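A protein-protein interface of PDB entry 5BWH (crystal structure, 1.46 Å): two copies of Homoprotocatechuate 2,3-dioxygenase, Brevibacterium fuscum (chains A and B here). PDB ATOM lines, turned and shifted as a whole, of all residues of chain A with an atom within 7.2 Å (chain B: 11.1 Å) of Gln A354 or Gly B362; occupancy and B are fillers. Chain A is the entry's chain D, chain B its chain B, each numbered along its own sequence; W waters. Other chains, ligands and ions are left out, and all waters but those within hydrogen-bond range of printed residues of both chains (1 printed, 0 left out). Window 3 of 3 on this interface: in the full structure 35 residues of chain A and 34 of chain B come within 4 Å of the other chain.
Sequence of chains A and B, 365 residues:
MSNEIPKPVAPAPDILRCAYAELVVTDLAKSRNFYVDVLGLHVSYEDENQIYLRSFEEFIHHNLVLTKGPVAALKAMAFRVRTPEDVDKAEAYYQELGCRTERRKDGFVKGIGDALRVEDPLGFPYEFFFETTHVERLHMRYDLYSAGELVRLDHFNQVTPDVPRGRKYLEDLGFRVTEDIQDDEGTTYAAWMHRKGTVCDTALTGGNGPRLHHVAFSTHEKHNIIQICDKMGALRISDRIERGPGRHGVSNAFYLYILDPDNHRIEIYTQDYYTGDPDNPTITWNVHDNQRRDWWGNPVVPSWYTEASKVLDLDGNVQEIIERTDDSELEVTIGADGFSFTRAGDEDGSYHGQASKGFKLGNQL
No residue of chain B comes within 4 Å of Gly A335. No residue of chain B comes within 4 Å of Ala A336. Phe A339 touches none of the printed residues of chain B. No residue of chain B comes within 4 Å of Gly A353. Of the printed residues of chain B, Gln A354 touches Gly B362. No residue of chain B comes within 4 Å of Ala A355. No residue of chain B comes within 4 Å of Ser A356. Of the printed residues of chain B, Leu A361 touches Gly B358 and Lys B360. Of the printed residues of chain A, Val B301 touches Lys A357 and Phe A359. Printed residues of chain A within 4 Å of Phe B359: Phe A359 and Lys A360. Printed residues of chain A within 4 Å of Leu B361: Lys A360. Printed residues of chain A within 4 Å of Gly B362: Gln A354, Gly A358 and Lys A360. The nearest residue of chain B that does not touch Gln A354 is Leu B361 (6.2 Å). The nearest printed residue of chain A that does not touch Gly B362 is Phe A359 (4.2 Å).
Of the 20 printed residues of chain B, 9 touch a printed residue of chain A. Printed residues of chain B that touch a printed residue of chain A: Pro B299, Val B300, Val B301, Pro B302, Gly B358, Phe B359, Lys B360, Leu B361 and Gly B362. Of the 20 printed residues of chain A, 6 touch a printed residue of chain B. Printed residues of chain A that touch a printed residue of chain B: Gln A354, Lys A357, Gly A358, Phe A359, Lys A360 and Leu A361. Hydrophobic or aromatic side chains of chain A within 4 Å of the printed part of chain B: Phe A359. Among the printed residues, no Asp or Glu carboxylate lies within 4 Å of a Lys or Arg side-chain nitrogen of the other chain.
The backbone carbonyl oxygen (O) of Lys B360 is in hydrogen-bond range of the backbone NH (N) of Lys A360. N of Gly B362 is in hydrogen-bond range of O of Gly A358, 3.0 Å away.
Water W1 bridges the backbone NH (N) of Ser B303 (3.0 Å) and the backbone carbonyl oxygen (O) of Lys A357 (3.3 Å).
Among the printed residues, pairs that only touch across the chains: Lys A357 with Val B301 (3.4 Å), Lys A360 with Leu B361 (3.4 Å), Phe A359 with Lys B360 (3.4 Å), Lys A360 with Phe B359 (3.5 Å), Phe A359 with Pro B299 (3.6 Å), Phe A359 with Phe B359 (3.7 Å), Phe A359 with Val B301 (3.7 Å), Leu A361 with Lys B360 (3.8 Å), Gln A354 with Gly B362 (3.9 Å), Leu A361 with Gly B358 (3.9 Å), Gly A358 with Pro B302 (3.95 Å), Phe A359 with Pro B302 (3.98 Å), Lys A360 with Gly B362 (3.99 Å) and Phe A359 with Val B300 (3.997 Å).
Phe B359 touches its own counterpart, Phe A359. Phe A359 touches Lys B360, and with the chains exchanged Lys A360 touches Phe B359. Lys A360 touches Leu B361, and with the chains exchanged Leu A361 touches Lys B360. Leu A361 touches Gly B358, but with the chains exchanged Gly A358 does not touch Leu B361 (4.1 Å). Positions printed for both chains: 334, 335, 336, 353, 354, 355, 356, 358, 359, 360 and 361. Of the 16 pairs that touch across the chains among the printed residues, 6 have their exchanged pair printed and touching as well.
The backbone carbonyl oxygen of Pro B302 is in hydrogen-bond range of the side-chain hydroxyl of Thr B306 (3.4 Å).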
ATOM      1  N   THR A 333      37.000   8.596  -9.645  1.00  0.00           N
ATOM      2  CA  THR A 333      35.776   7.991 -10.178  1.00  0.00           C
ATOM      3  C   THR A 333      35.012   7.081  -9.210  1.00  0.00           C
ATOM      4  O   THR A 333      33.786   7.118  -9.182  1.00  0.00           O
ATOM      5  CB  THR A 333      36.062   7.199 -11.476  1.00  0.00           C
ATOM      6  OG1 THR A 333      36.966   6.122 -11.222  1.00  0.00           O
ATOM      7  CG2 THR A 333      36.661   8.103 -12.507  1.00  0.00           C
ATOM      8  N   ILE A 334      35.717   6.224  -8.474  1.00  0.00           N
ATOM      9  CA  ILE A 334      35.049   5.204  -7.655  1.00  0.00           C
ATOM     10  C   ILE A 334      35.455   5.191  -6.173  1.00  0.00           C
ATOM     11  O   ILE A 334      34.859   4.439  -5.385  1.00  0.00           O
ATOM     12  CB  ILE A 334      35.200   3.774  -8.232  1.00  0.00           C
ATOM     13  CG1 ILE A 334      36.671   3.339  -8.337  1.00  0.00           C
ATOM     14  CG2 ILE A 334      34.539   3.674  -9.602  1.00  0.00           C
ATOM     15  CD1 ILE A 334      36.872   1.871  -8.714  1.00  0.00           C
ATOM     16  N   GLY A 335      36.420   6.034  -5.805  1.00  0.00           N
ATOM     17  CA  GLY A 335      36.805   6.210  -4.406  1.00  0.00           C
ATOM     18  C   GLY A 335      35.758   6.951  -3.597  1.00  0.00           C
ATOM     19  O   GLY A 335      34.735   7.383  -4.131  1.00  0.00           O
ATOM     20  N   ALA A 336      36.013   7.122  -2.302  1.00  0.00           N
ATOM     21  CA  ALA A 336      35.033   7.761  -1.422  1.00  0.00           C
ATOM     22  C   ALA A 336      34.707   9.206  -1.842  1.00  0.00           C
ATOM     23  O   ALA A 336      33.602   9.685  -1.569  1.00  0.00           O
ATOM     24  CB  ALA A 336      35.492   7.716   0.037  1.00  0.00           C
ATOM     25  N   ASP A 337      35.659   9.891  -2.488  1.00  0.00           N
ATOM     26  CA  ASP A 337      35.438  11.239  -3.048  1.00  0.00           C
ATOM     27  C   ASP A 337      35.261  11.279  -4.558  1.00  0.00           C
ATOM     28  O   ASP A 337      35.296  12.352  -5.165  1.00  0.00           O
ATOM     29  CB  ASP A 337      36.616  12.131  -2.696  1.00  0.00           C
ATOM     30  CG  ASP A 337      36.605  12.533  -1.254  1.00  0.00           C
ATOM     31  OD1 ASP A 337      35.497  12.627  -0.683  1.00  0.00           O
ATOM     32  OD2 ASP A 337      37.695  12.735  -0.699  1.00  0.00           O
ATOM     33  N   GLY A 338      35.070  10.110  -5.149  1.00  0.00           N
ATOM     34  CA  GLY A 338      35.012   9.964  -6.603  1.00  0.00           C
ATOM     35  C   GLY A 338      33.610  10.250  -7.082  1.00  0.00           C
ATOM     36  O   GLY A 338      32.652  10.241  -6.304  1.00  0.00           O
ATOM     37  N   PHE A 339      33.464  10.486  -8.380  1.00  0.00           N
ATOM     38  CA  PHE A 339      32.152  10.430  -8.981  1.00  0.00           C
ATOM     39  C   PHE A 339      32.237  10.059 -10.457  1.00  0.00           C
ATOM     40  O   PHE A 339      33.264  10.220 -11.110  1.00  0.00           O
ATOM     41  CB  PHE A 339      31.391  11.737  -8.768  1.00  0.00           C
ATOM     42  CG  PHE A 339      31.738  12.810  -9.749  1.00  0.00           C
ATOM     43  CD1 PHE A 339      32.856  13.604  -9.558  1.00  0.00           C
ATOM     44  CD2 PHE A 339      30.942  13.017 -10.866  1.00  0.00           C
ATOM     45  CE1 PHE A 339      33.179  14.597 -10.468  1.00  0.00           C
ATOM     46  CE2 PHE A 339      31.254  14.011 -11.783  1.00  0.00           C
ATOM     47  CZ  PHE A 339      32.384  14.792 -11.588  1.00  0.00           C
ATOM     48  N   SER A 340      31.125   9.551 -10.963  1.00  0.00           N
ATOM     49  CA  SER A 340      30.956   9.350 -12.393  1.00  0.00           C
ATOM     50  C   SER A 340      29.501   9.615 -12.781  1.00  0.00           C
ATOM     51  O   SER A 340      28.588   9.620 -11.946  1.00  0.00           O
ATOM     52  CB  SER A 340      31.385   7.936 -12.785  1.00  0.00           C
ATOM     53  OG  SER A 340      30.481   6.937 -12.330  1.00  0.00           O
ATOM     54  N   SER A 350      24.056   9.124 -11.868  1.00  0.00           N
ATOM     55  CA  SER A 350      25.380   9.457 -11.377  1.00  0.00           C
ATOM     56  C   SER A 350      25.682   8.771 -10.053  1.00  0.00           C
ATOM     57  O   SER A 350      24.778   8.446  -9.273  1.00  0.00           O
ATOM     58  CB  SER A 350      25.544  10.971 -11.236  1.00  0.00           C
ATOM     59  OG  SER A 350      24.862  11.466 -10.098  1.00  0.00           O
ATOM     60  N   TYR A 351      26.976   8.596  -9.806  1.00  0.00           N
ATOM     61  CA  TYR A 351      27.494   7.792  -8.690  1.00  0.00           C
ATOM     62  C   TYR A 351      28.472   8.651  -7.942  1.00  0.00           C
ATOM     63  O   TYR A 351      29.360   9.245  -8.539  1.00  0.00           O
ATOM     64  CB  TYR A 351      28.129   6.493  -9.194  1.00  0.00           C
ATOM     65  CG  TYR A 351      27.163   5.721 -10.040  1.00  0.00           C
ATOM     66  CD1 TYR A 351      26.074   5.052  -9.478  1.00  0.00           C
ATOM     67  CD2 TYR A 351      27.297   5.713 -11.427  1.00  0.00           C
ATOM     68  CE1 TYR A 351      25.150   4.384 -10.277  1.00  0.00           C
ATOM     69  CE2 TYR A 351      26.378   5.060 -12.238  1.00  0.00           C
ATOM     70  CZ  TYR A 351      25.318   4.384 -11.668  1.00  0.00           C
ATOM     71  OH  TYR A 351      24.415   3.728 -12.480  1.00  0.00           O
ATOM     72  N   HIS A 352      28.277   8.756  -6.628  1.00  0.00           N
ATOM     73  CA  HIS A 352      29.153   9.582  -5.797  1.00  0.00           C
ATOM     74  C   HIS A 352      29.703   8.755  -4.647  1.00  0.00           C
ATOM     75  O   HIS A 352      28.954   8.171  -3.871  1.00  0.00           O
ATOM     76  CB  HIS A 352      28.408  10.800  -5.258  1.00  0.00           C
ATOM     77  CG  HIS A 352      27.844  11.678  -6.330  1.00  0.00           C
ATOM     78  ND1 HIS A 352      28.567  12.688  -6.925  1.00  0.00           N
ATOM     79  CD2 HIS A 352      26.635  11.673  -6.940  1.00  0.00           C
ATOM     80  CE1 HIS A 352      27.827  13.268  -7.855  1.00  0.00           C
ATOM     81  NE2 HIS A 352      26.648  12.675  -7.877  1.00  0.00           N
ATOM     82  N   GLY A 353      31.024   8.712  -4.546  1.00  0.00           N
ATOM     83  CA  GLY A 353      31.692   7.990  -3.465  1.00  0.00           C
ATOM     84  C   GLY A 353      31.598   6.482  -3.548  1.00  0.00           C
ATOM     85  O   GLY A 353      31.904   5.763  -2.576  1.00  0.00           O
ATOM     86  N   GLN A 354      31.202   5.988  -4.714  1.00  0.00           N
ATOM     87  CA  GLN A 354      31.135   4.568  -4.934  1.00  0.00           C
ATOM     88  C   GLN A 354      31.092   4.312  -6.418  1.00  0.00           C
ATOM     89  O   GLN A 354      31.028   5.250  -7.210  1.00  0.00           O
ATOM     90  CB  GLN A 354      29.938   3.945  -4.233  1.00  0.00           C
ATOM     91  CG  GLN A 354      28.561   4.422  -4.649  1.00  0.00           C
ATOM     92  CD  GLN A 354      27.486   3.804  -3.754  1.00  0.00           C
ATOM     93  OE1 GLN A 354      27.525   3.955  -2.539  1.00  0.00           O
ATOM     94  NE2 GLN A 354      26.569   3.060  -4.343  1.00  0.00           N
ATOM     95  N   ALA A 355      31.156   3.043  -6.783  1.00  0.00           N
ATOM     96  CA  ALA A 355      31.094   2.652  -8.167  1.00  0.00           C
ATOM     97  C   ALA A 355      29.649   2.573  -8.636  1.00  0.00           C
ATOM     98  O   ALA A 355      28.699   2.746  -7.868  1.00  0.00           O
ATOM     99  CB  ALA A 355      31.818   1.330  -8.340  1.00  0.00           C
ATOM    100  N   SER A 356      29.494   2.333  -9.929  1.00  0.00           N
ATOM    101  CA  SER A 356      28.198   2.091 -10.508  1.00  0.00           C
ATOM    102  C   SER A 356      27.574   0.798  -9.977  1.00  0.00           C
ATOM    103  O   SER A 356      28.264  -0.068  -9.409  1.00  0.00           O
ATOM    104  CB  SER A 356      28.337   2.058 -12.031  1.00  0.00           C
ATOM    105  OG  SER A 356      29.327   1.113 -12.393  1.00  0.00           O
ATOM    106  N   LYS A 357      26.264   0.671 -10.195  1.00  0.00           N
ATOM    107  CA  LYS A 357      25.527  -0.584 -10.029  1.00  0.00           C
ATOM    108  C   LYS A 357      25.434  -1.039  -8.564  1.00  0.00           C
ATOM    109  O   LYS A 357      25.060  -2.184  -8.292  1.00  0.00           O
ATOM    110  CB  LYS A 357      26.068  -1.742 -10.923  1.00  0.00           C
ATOM    111  CG  LYS A 357      26.519  -1.390 -12.354  1.00  0.00           C
ATOM    112  CD  LYS A 357      25.403  -1.255 -13.366  1.00  0.00           C
ATOM    113  CE  LYS A 357      25.866  -1.133 -14.816  1.00  0.00           C
ATOM    114  NZ  LYS A 357      24.966  -0.216 -15.612  1.00  0.00           N
ATOM    115  N   GLY A 358      25.759  -0.161  -7.618  1.00  0.00           N
ATOM    116  CA  GLY A 358      25.431  -0.373  -6.205  1.00  0.00           C
ATOM    117  C   GLY A 358      26.582  -0.872  -5.341  1.00  0.00           C
ATOM    118  O   GLY A 358      26.386  -1.261  -4.177  1.00  0.00           O
ATOM    119  N   PHE A 359      27.783  -0.867  -5.892  1.00  0.00           N
ATOM    120  CA  PHE A 359      28.973  -1.342  -5.174  1.00  0.00           C
ATOM    121  C   PHE A 359      29.846  -0.184  -4.705  1.00  0.00           C
ATOM    122  O   PHE A 359      29.936   0.842  -5.367  1.00  0.00           O
ATOM    123  CB  PHE A 359      29.809  -2.241  -6.082  1.00  0.00           C
ATOM    124  CG  PHE A 359      29.118  -3.519  -6.454  1.00  0.00           C
ATOM    125  CD1 PHE A 359      28.734  -4.431  -5.473  1.00  0.00           C
ATOM    126  CD2 PHE A 359      28.817  -3.792  -7.788  1.00  0.00           C
ATOM    127  CE1 PHE A 359      28.081  -5.613  -5.825  1.00  0.00           C
ATOM    128  CE2 PHE A 359      28.172  -4.961  -8.138  1.00  0.00           C
ATOM    129  CZ  PHE A 359      27.802  -5.870  -7.153  1.00  0.00           C
ATOM    130  N   LYS A 360      30.520  -0.378  -3.581  1.00  0.00           N
ATOM    131  CA  LYS A 360      31.666   0.436  -3.221  1.00  0.00           C
ATOM    132  C   LYS A 360      32.936  -0.412  -3.182  1.00  0.00           C
ATOM    133  O   LYS A 360      32.882  -1.639  -3.364  1.00  0.00           O
ATOM    134  CB  LYS A 360      31.414   1.120  -1.892  1.00  0.00           C
ATOM    135  CG  LYS A 360      31.475   0.204  -0.696  1.00  0.00           C
ATOM    136  CD  LYS A 360      31.395   1.013   0.583  1.00  0.00           C
ATOM    137  CE  LYS A 360      31.579   0.126   1.801  1.00  0.00           C
ATOM    138  NZ  LYS A 360      31.669   0.901   3.069  1.00  0.00           N
ATOM    139  N   LEU A 361      34.074   0.244  -2.966  1.00  0.00           N
ATOM    140  CA  LEU A 361      35.360  -0.441  -2.995  1.00  0.00           C
ATOM    141  C   LEU A 361      35.370  -1.442  -1.854  1.00  0.00           C
ATOM    142  O   LEU A 361      34.935  -1.117  -0.744  1.00  0.00           O
ATOM    143  CB  LEU A 361      36.520   0.530  -2.802  1.00  0.00           C
ATOM    144  CG  LEU A 361      36.741   1.671  -3.793  1.00  0.00           C
ATOM    145  CD1 LEU A 361      37.747   2.657  -3.201  1.00  0.00           C
ATOM    146  CD2 LEU A 361      37.234   1.147  -5.115  1.00  0.00           C
ATOM    147  N   PRO B 299      29.772 -10.301  -9.253  1.00  0.00           N
ATOM    148  CA  PRO B 299      28.946 -10.121  -8.077  1.00  0.00           C
ATOM    149  C   PRO B 299      27.505  -9.765  -8.439  1.00  0.00           C
ATOM    150  O   PRO B 299      27.243  -9.139  -9.465  1.00  0.00           O
ATOM    151  CB  PRO B 299      29.658  -8.988  -7.326  1.00  0.00           C
ATOM    152  CG  PRO B 299      30.317  -8.208  -8.397  1.00  0.00           C
ATOM    153  CD  PRO B 299      30.776  -9.227  -9.380  1.00  0.00           C
ATOM    154  N   VAL B 300      26.576 -10.217  -7.611  1.00  0.00           N
ATOM    155  CA  VAL B 300      25.155  -9.918  -7.801  1.00  0.00           C
ATOM    156  C   VAL B 300      24.856  -8.599  -7.105  1.00  0.00           C
ATOM    157  O   VAL B 300      25.038  -8.471  -5.899  1.00  0.00           O
ATOM    158  CB  VAL B 300      24.248 -11.039  -7.257  1.00  0.00           C
ATOM    159  CG1 VAL B 300      22.776 -10.684  -7.402  1.00  0.00           C
ATOM    160  CG2 VAL B 300      24.568 -12.339  -7.963  1.00  0.00           C
ATOM    161  N   VAL B 301      24.393  -7.621  -7.888  1.00  0.00           N
ATOM    162  CA  VAL B 301      24.131  -6.290  -7.387  1.00  0.00           C
ATOM    163  C   VAL B 301      23.030  -6.347  -6.313  1.00  0.00           C
ATOM    164  O   VAL B 301      22.049  -7.089  -6.457  1.00  0.00           O
ATOM    165  CB  VAL B 301      23.779  -5.314  -8.546  1.00  0.00           C
ATOM    166  CG1 VAL B 301      24.805  -5.417  -9.683  1.00  0.00           C
ATOM    167  CG2 VAL B 301      22.421  -5.605  -9.105  1.00  0.00           C
ATOM    168  N   PRO B 302      23.199  -5.595  -5.209  1.00  0.00           N
ATOM    169  CA  PRO B 302      22.248  -5.718  -4.103  1.00  0.00           C
ATOM    170  C   PRO B 302      20.779  -5.427  -4.493  1.00  0.00           C
ATOM    171  O   PRO B 302      19.860  -6.057  -3.950  1.00  0.00           O
ATOM    172  CB  PRO B 302      22.759  -4.717  -3.061  1.00  0.00           C
ATOM    173  CG  PRO B 302      24.181  -4.454  -3.432  1.00  0.00           C
ATOM    174  CD  PRO B 302      24.323  -4.692  -4.896  1.00  0.00           C
ATOM    175  N   SER B 303      20.551  -4.510  -5.436  1.00  0.00           N
ATOM    176  CA  SER B 303      19.185  -4.220  -5.865  1.00  0.00           C
ATOM    177  C   SER B 303      18.469  -5.429  -6.431  1.00  0.00           C
ATOM    178  O   SER B 303      17.244  -5.515  -6.358  1.00  0.00           O
ATOM    179  CB  SER B 303      19.143  -3.094  -6.895  1.00  0.00           C
ATOM    180  OG  SER B 303      19.826  -3.453  -8.093  1.00  0.00           O
ATOM    181  N   THR B 306      16.923  -6.910  -3.414  1.00  0.00           N
ATOM    182  CA  THR B 306      16.052  -6.094  -2.570  1.00  0.00           C
ATOM    183  C   THR B 306      14.844  -5.492  -3.307  1.00  0.00           C
ATOM    184  O   THR B 306      13.825  -5.218  -2.688  1.00  0.00           O
ATOM    185  CB  THR B 306      16.835  -4.981  -1.854  1.00  0.00           C
ATOM    186  OG1 THR B 306      17.364  -4.076  -2.814  1.00  0.00           O
ATOM    187  CG2 THR B 306      17.980  -5.562  -1.030  1.00  0.00           C
ATOM    188  N   LEU B 330      21.126 -12.352   0.097  1.00  0.00           N
ATOM    189  CA  LEU B 330      22.034 -11.229   0.123  1.00  0.00           C
ATOM    190  C   LEU B 330      22.914 -11.312   1.373  1.00  0.00           C
ATOM    191  O   LEU B 330      24.137 -11.279   1.275  1.00  0.00           O
ATOM    192  CB  LEU B 330      21.241  -9.911   0.094  1.00  0.00           C
ATOM    193  CG  LEU B 330      22.093  -8.624   0.093  1.00  0.00           C
ATOM    194  CD1 LEU B 330      21.311  -7.461  -0.472  1.00  0.00           C
ATOM    195  CD2 LEU B 330      22.616  -8.301   1.487  1.00  0.00           C
ATOM    196  N   GLU B 331      22.293 -11.452   2.545  1.00  0.00           N
ATOM    197  CA  GLU B 331      23.058 -11.405   3.786  1.00  0.00           C
ATOM    198  C   GLU B 331      24.068 -12.540   3.882  1.00  0.00           C
ATOM    199  O   GLU B 331      25.211 -12.318   4.298  1.00  0.00           O
ATOM    200  CB  GLU B 331      22.129 -11.381   5.012  1.00  0.00           C
ATOM    201  CG  GLU B 331      21.303 -10.109   5.152  1.00  0.00           C
ATOM    202  CD  GLU B 331      22.119  -8.832   5.367  1.00  0.00           C
ATOM    203  OE1 GLU B 331      23.340  -8.899   5.647  1.00  0.00           O
ATOM    204  OE2 GLU B 331      21.514  -7.733   5.277  1.00  0.00           O
ATOM    205  N   ILE B 334      26.896 -11.897   0.438  1.00  0.00           N
ATOM    206  CA  ILE B 334      27.639 -10.655   0.214  1.00  0.00           C
ATOM    207  C   ILE B 334      27.515  -9.632   1.341  1.00  0.00           C
ATOM    208  O   ILE B 334      28.177  -8.579   1.300  1.00  0.00           O
ATOM    209  CB  ILE B 334      27.274  -9.997  -1.147  1.00  0.00           C
ATOM    210  CG1 ILE B 334      25.793  -9.585  -1.225  1.00  0.00           C
ATOM    211  CG2 ILE B 334      27.612 -10.956  -2.277  1.00  0.00           C
ATOM    212  CD1 ILE B 334      25.432  -8.826  -2.507  1.00  0.00           C
ATOM    213  N   GLY B 335      26.704  -9.945   2.348  1.00  0.00           N
ATOM    214  CA  GLY B 335      26.557  -9.097   3.514  1.00  0.00           C
ATOM    215  C   GLY B 335      27.735  -9.224   4.458  1.00  0.00           C
ATOM    216  O   GLY B 335      28.685  -9.974   4.193  1.00  0.00           O
ATOM    217  N   ALA B 336      27.649  -8.506   5.575  1.00  0.00           N
ATOM    218  CA  ALA B 336      28.778  -8.352   6.502  1.00  0.00           C
ATOM    219  C   ALA B 336      29.265  -9.666   7.102  1.00  0.00           C
ATOM    220  O   ALA B 336      30.444  -9.804   7.388  1.00  0.00           O
ATOM    221  CB  ALA B 336      28.400  -7.389   7.615  1.00  0.00           C
ATOM    222  N   GLY B 353      32.488 -11.617   4.012  1.00  0.00           N
ATOM    223  CA  GLY B 353      31.914 -10.309   4.343  1.00  0.00           C
ATOM    224  C   GLY B 353      31.981  -9.281   3.233  1.00  0.00           C
ATOM    225  O   GLY B 353      31.960  -8.084   3.492  1.00  0.00           O
ATOM    226  N   GLN B 354      32.052  -9.743   1.992  1.00  0.00           N
ATOM    227  CA  GLN B 354      31.991  -8.848   0.857  1.00  0.00           C
ATOM    228  C   GLN B 354      31.663  -9.607  -0.410  1.00  0.00           C
ATOM    229  O   GLN B 354      31.548 -10.824  -0.398  1.00  0.00           O
ATOM    230  CB  GLN B 354      33.283  -8.056   0.701  1.00  0.00           C
ATOM    231  CG  GLN B 354      34.501  -8.794   0.194  1.00  0.00           C
ATOM    232  CD  GLN B 354      35.608  -7.795  -0.132  1.00  0.00           C
ATOM    233  OE1 GLN B 354      36.252  -7.860  -1.173  1.00  0.00           O
ATOM    234  NE2 GLN B 354      35.777  -6.827   0.738  1.00  0.00           N
ATOM    235  N   ALA B 355      31.508  -8.865  -1.495  1.00  0.00           N
ATOM    236  CA  ALA B 355      31.201  -9.457  -2.768  1.00  0.00           C
ATOM    237  C   ALA B 355      32.488  -9.881  -3.481  1.00  0.00           C
ATOM    238  O   ALA B 355      33.591  -9.533  -3.068  1.00  0.00           O
ATOM    239  CB  ALA B 355      30.418  -8.467  -3.616  1.00  0.00           C
ATOM    240  N   SER B 356      32.321 -10.622  -4.571  1.00  0.00           N
ATOM    241  CA  SER B 356      33.437 -10.998  -5.431  1.00  0.00           C
ATOM    242  C   SER B 356      34.010  -9.797  -6.181  1.00  0.00           C
ATOM    243  O   SER B 356      33.389  -8.711  -6.226  1.00  0.00           O
ATOM    244  CB  SER B 356      32.991 -12.054  -6.431  1.00  0.00           C
ATOM    245  OG  SER B 356      31.905 -11.555  -7.195  1.00  0.00           O
ATOM    246  N   GLY B 358      36.304  -7.652  -5.819  1.00  0.00           N
ATOM    247  CA  GLY B 358      36.885  -6.477  -5.174  1.00  0.00           C
ATOM    248  C   GLY B 358      35.885  -5.421  -4.718  1.00  0.00           C
ATOM    249  O   GLY B 358      36.263  -4.277  -4.405  1.00  0.00           O
ATOM    250  N   PHE B 359      34.614  -5.806  -4.655  1.00  0.00           N
ATOM    251  CA  PHE B 359      33.535  -4.910  -4.287  1.00  0.00           C
ATOM    252  C   PHE B 359      32.904  -5.256  -2.935  1.00  0.00           C
ATOM    253  O   PHE B 359      32.946  -6.411  -2.486  1.00  0.00           O
ATOM    254  CB  PHE B 359      32.477  -4.914  -5.366  1.00  0.00           C
ATOM    255  CG  PHE B 359      32.950  -4.352  -6.672  1.00  0.00           C
ATOM    256  CD1 PHE B 359      33.340  -3.029  -6.779  1.00  0.00           C
ATOM    257  CD2 PHE B 359      33.005  -5.163  -7.806  1.00  0.00           C
ATOM    258  CE1 PHE B 359      33.757  -2.507  -8.014  1.00  0.00           C
ATOM    259  CE2 PHE B 359      33.410  -4.651  -9.017  1.00  0.00           C
ATOM    260  CZ  PHE B 359      33.808  -3.330  -9.114  1.00  0.00           C
ATOM    261  N   LYS B 360      32.342  -4.224  -2.307  1.00  0.00           N
ATOM    262  CA  LYS B 360      31.492  -4.333  -1.125  1.00  0.00           C
ATOM    263  C   LYS B 360      30.146  -3.694  -1.407  1.00  0.00           C
ATOM    264  O   LYS B 360      30.033  -2.870  -2.313  1.00  0.00           O
ATOM    265  CB  LYS B 360      32.133  -3.586   0.058  1.00  0.00           C
ATOM    266  CG  LYS B 360      32.900  -4.472   0.985  1.00  0.00           C
ATOM    267  CD  LYS B 360      33.388  -3.688   2.189  1.00  0.00           C
ATOM    268  CE  LYS B 360      33.852  -4.633   3.295  1.00  0.00           C
ATOM    269  NZ  LYS B 360      35.149  -4.217   3.895  1.00  0.00           N
ATOM    270  N   LEU B 361      29.138  -4.077  -0.634  1.00  0.00           N
ATOM    271  CA  LEU B 361      27.831  -3.398  -0.618  1.00  0.00           C
ATOM    272  C   LEU B 361      27.999  -1.878  -0.467  1.00  0.00           C
ATOM    273  O   LEU B 361      28.724  -1.444   0.423  1.00  0.00           O
ATOM    274  CB  LEU B 361      27.009  -3.901   0.579  1.00  0.00           C
ATOM    275  CG  LEU B 361      26.454  -5.323   0.634  1.00  0.00           C
ATOM    276  CD1 LEU B 361      25.709  -5.561   1.940  1.00  0.00           C
ATOM    277  CD2 LEU B 361      25.531  -5.587  -0.535  1.00  0.00           C
ATOM    278  N   GLY B 362      27.324  -1.072  -1.299  1.00  0.00           N
ATOM    279  CA  GLY B 362      27.243   0.384  -1.042  1.00  0.00           C
ATOM    280  C   GLY B 362      26.621   0.780   0.303  1.00  0.00           C
ATOM    281  O   GLY B 362      25.754   0.073   0.821  1.00  0.00           O
HETATM  282  O   HOH W   1      22.340  -2.365  -6.516  1.00  0.00           O
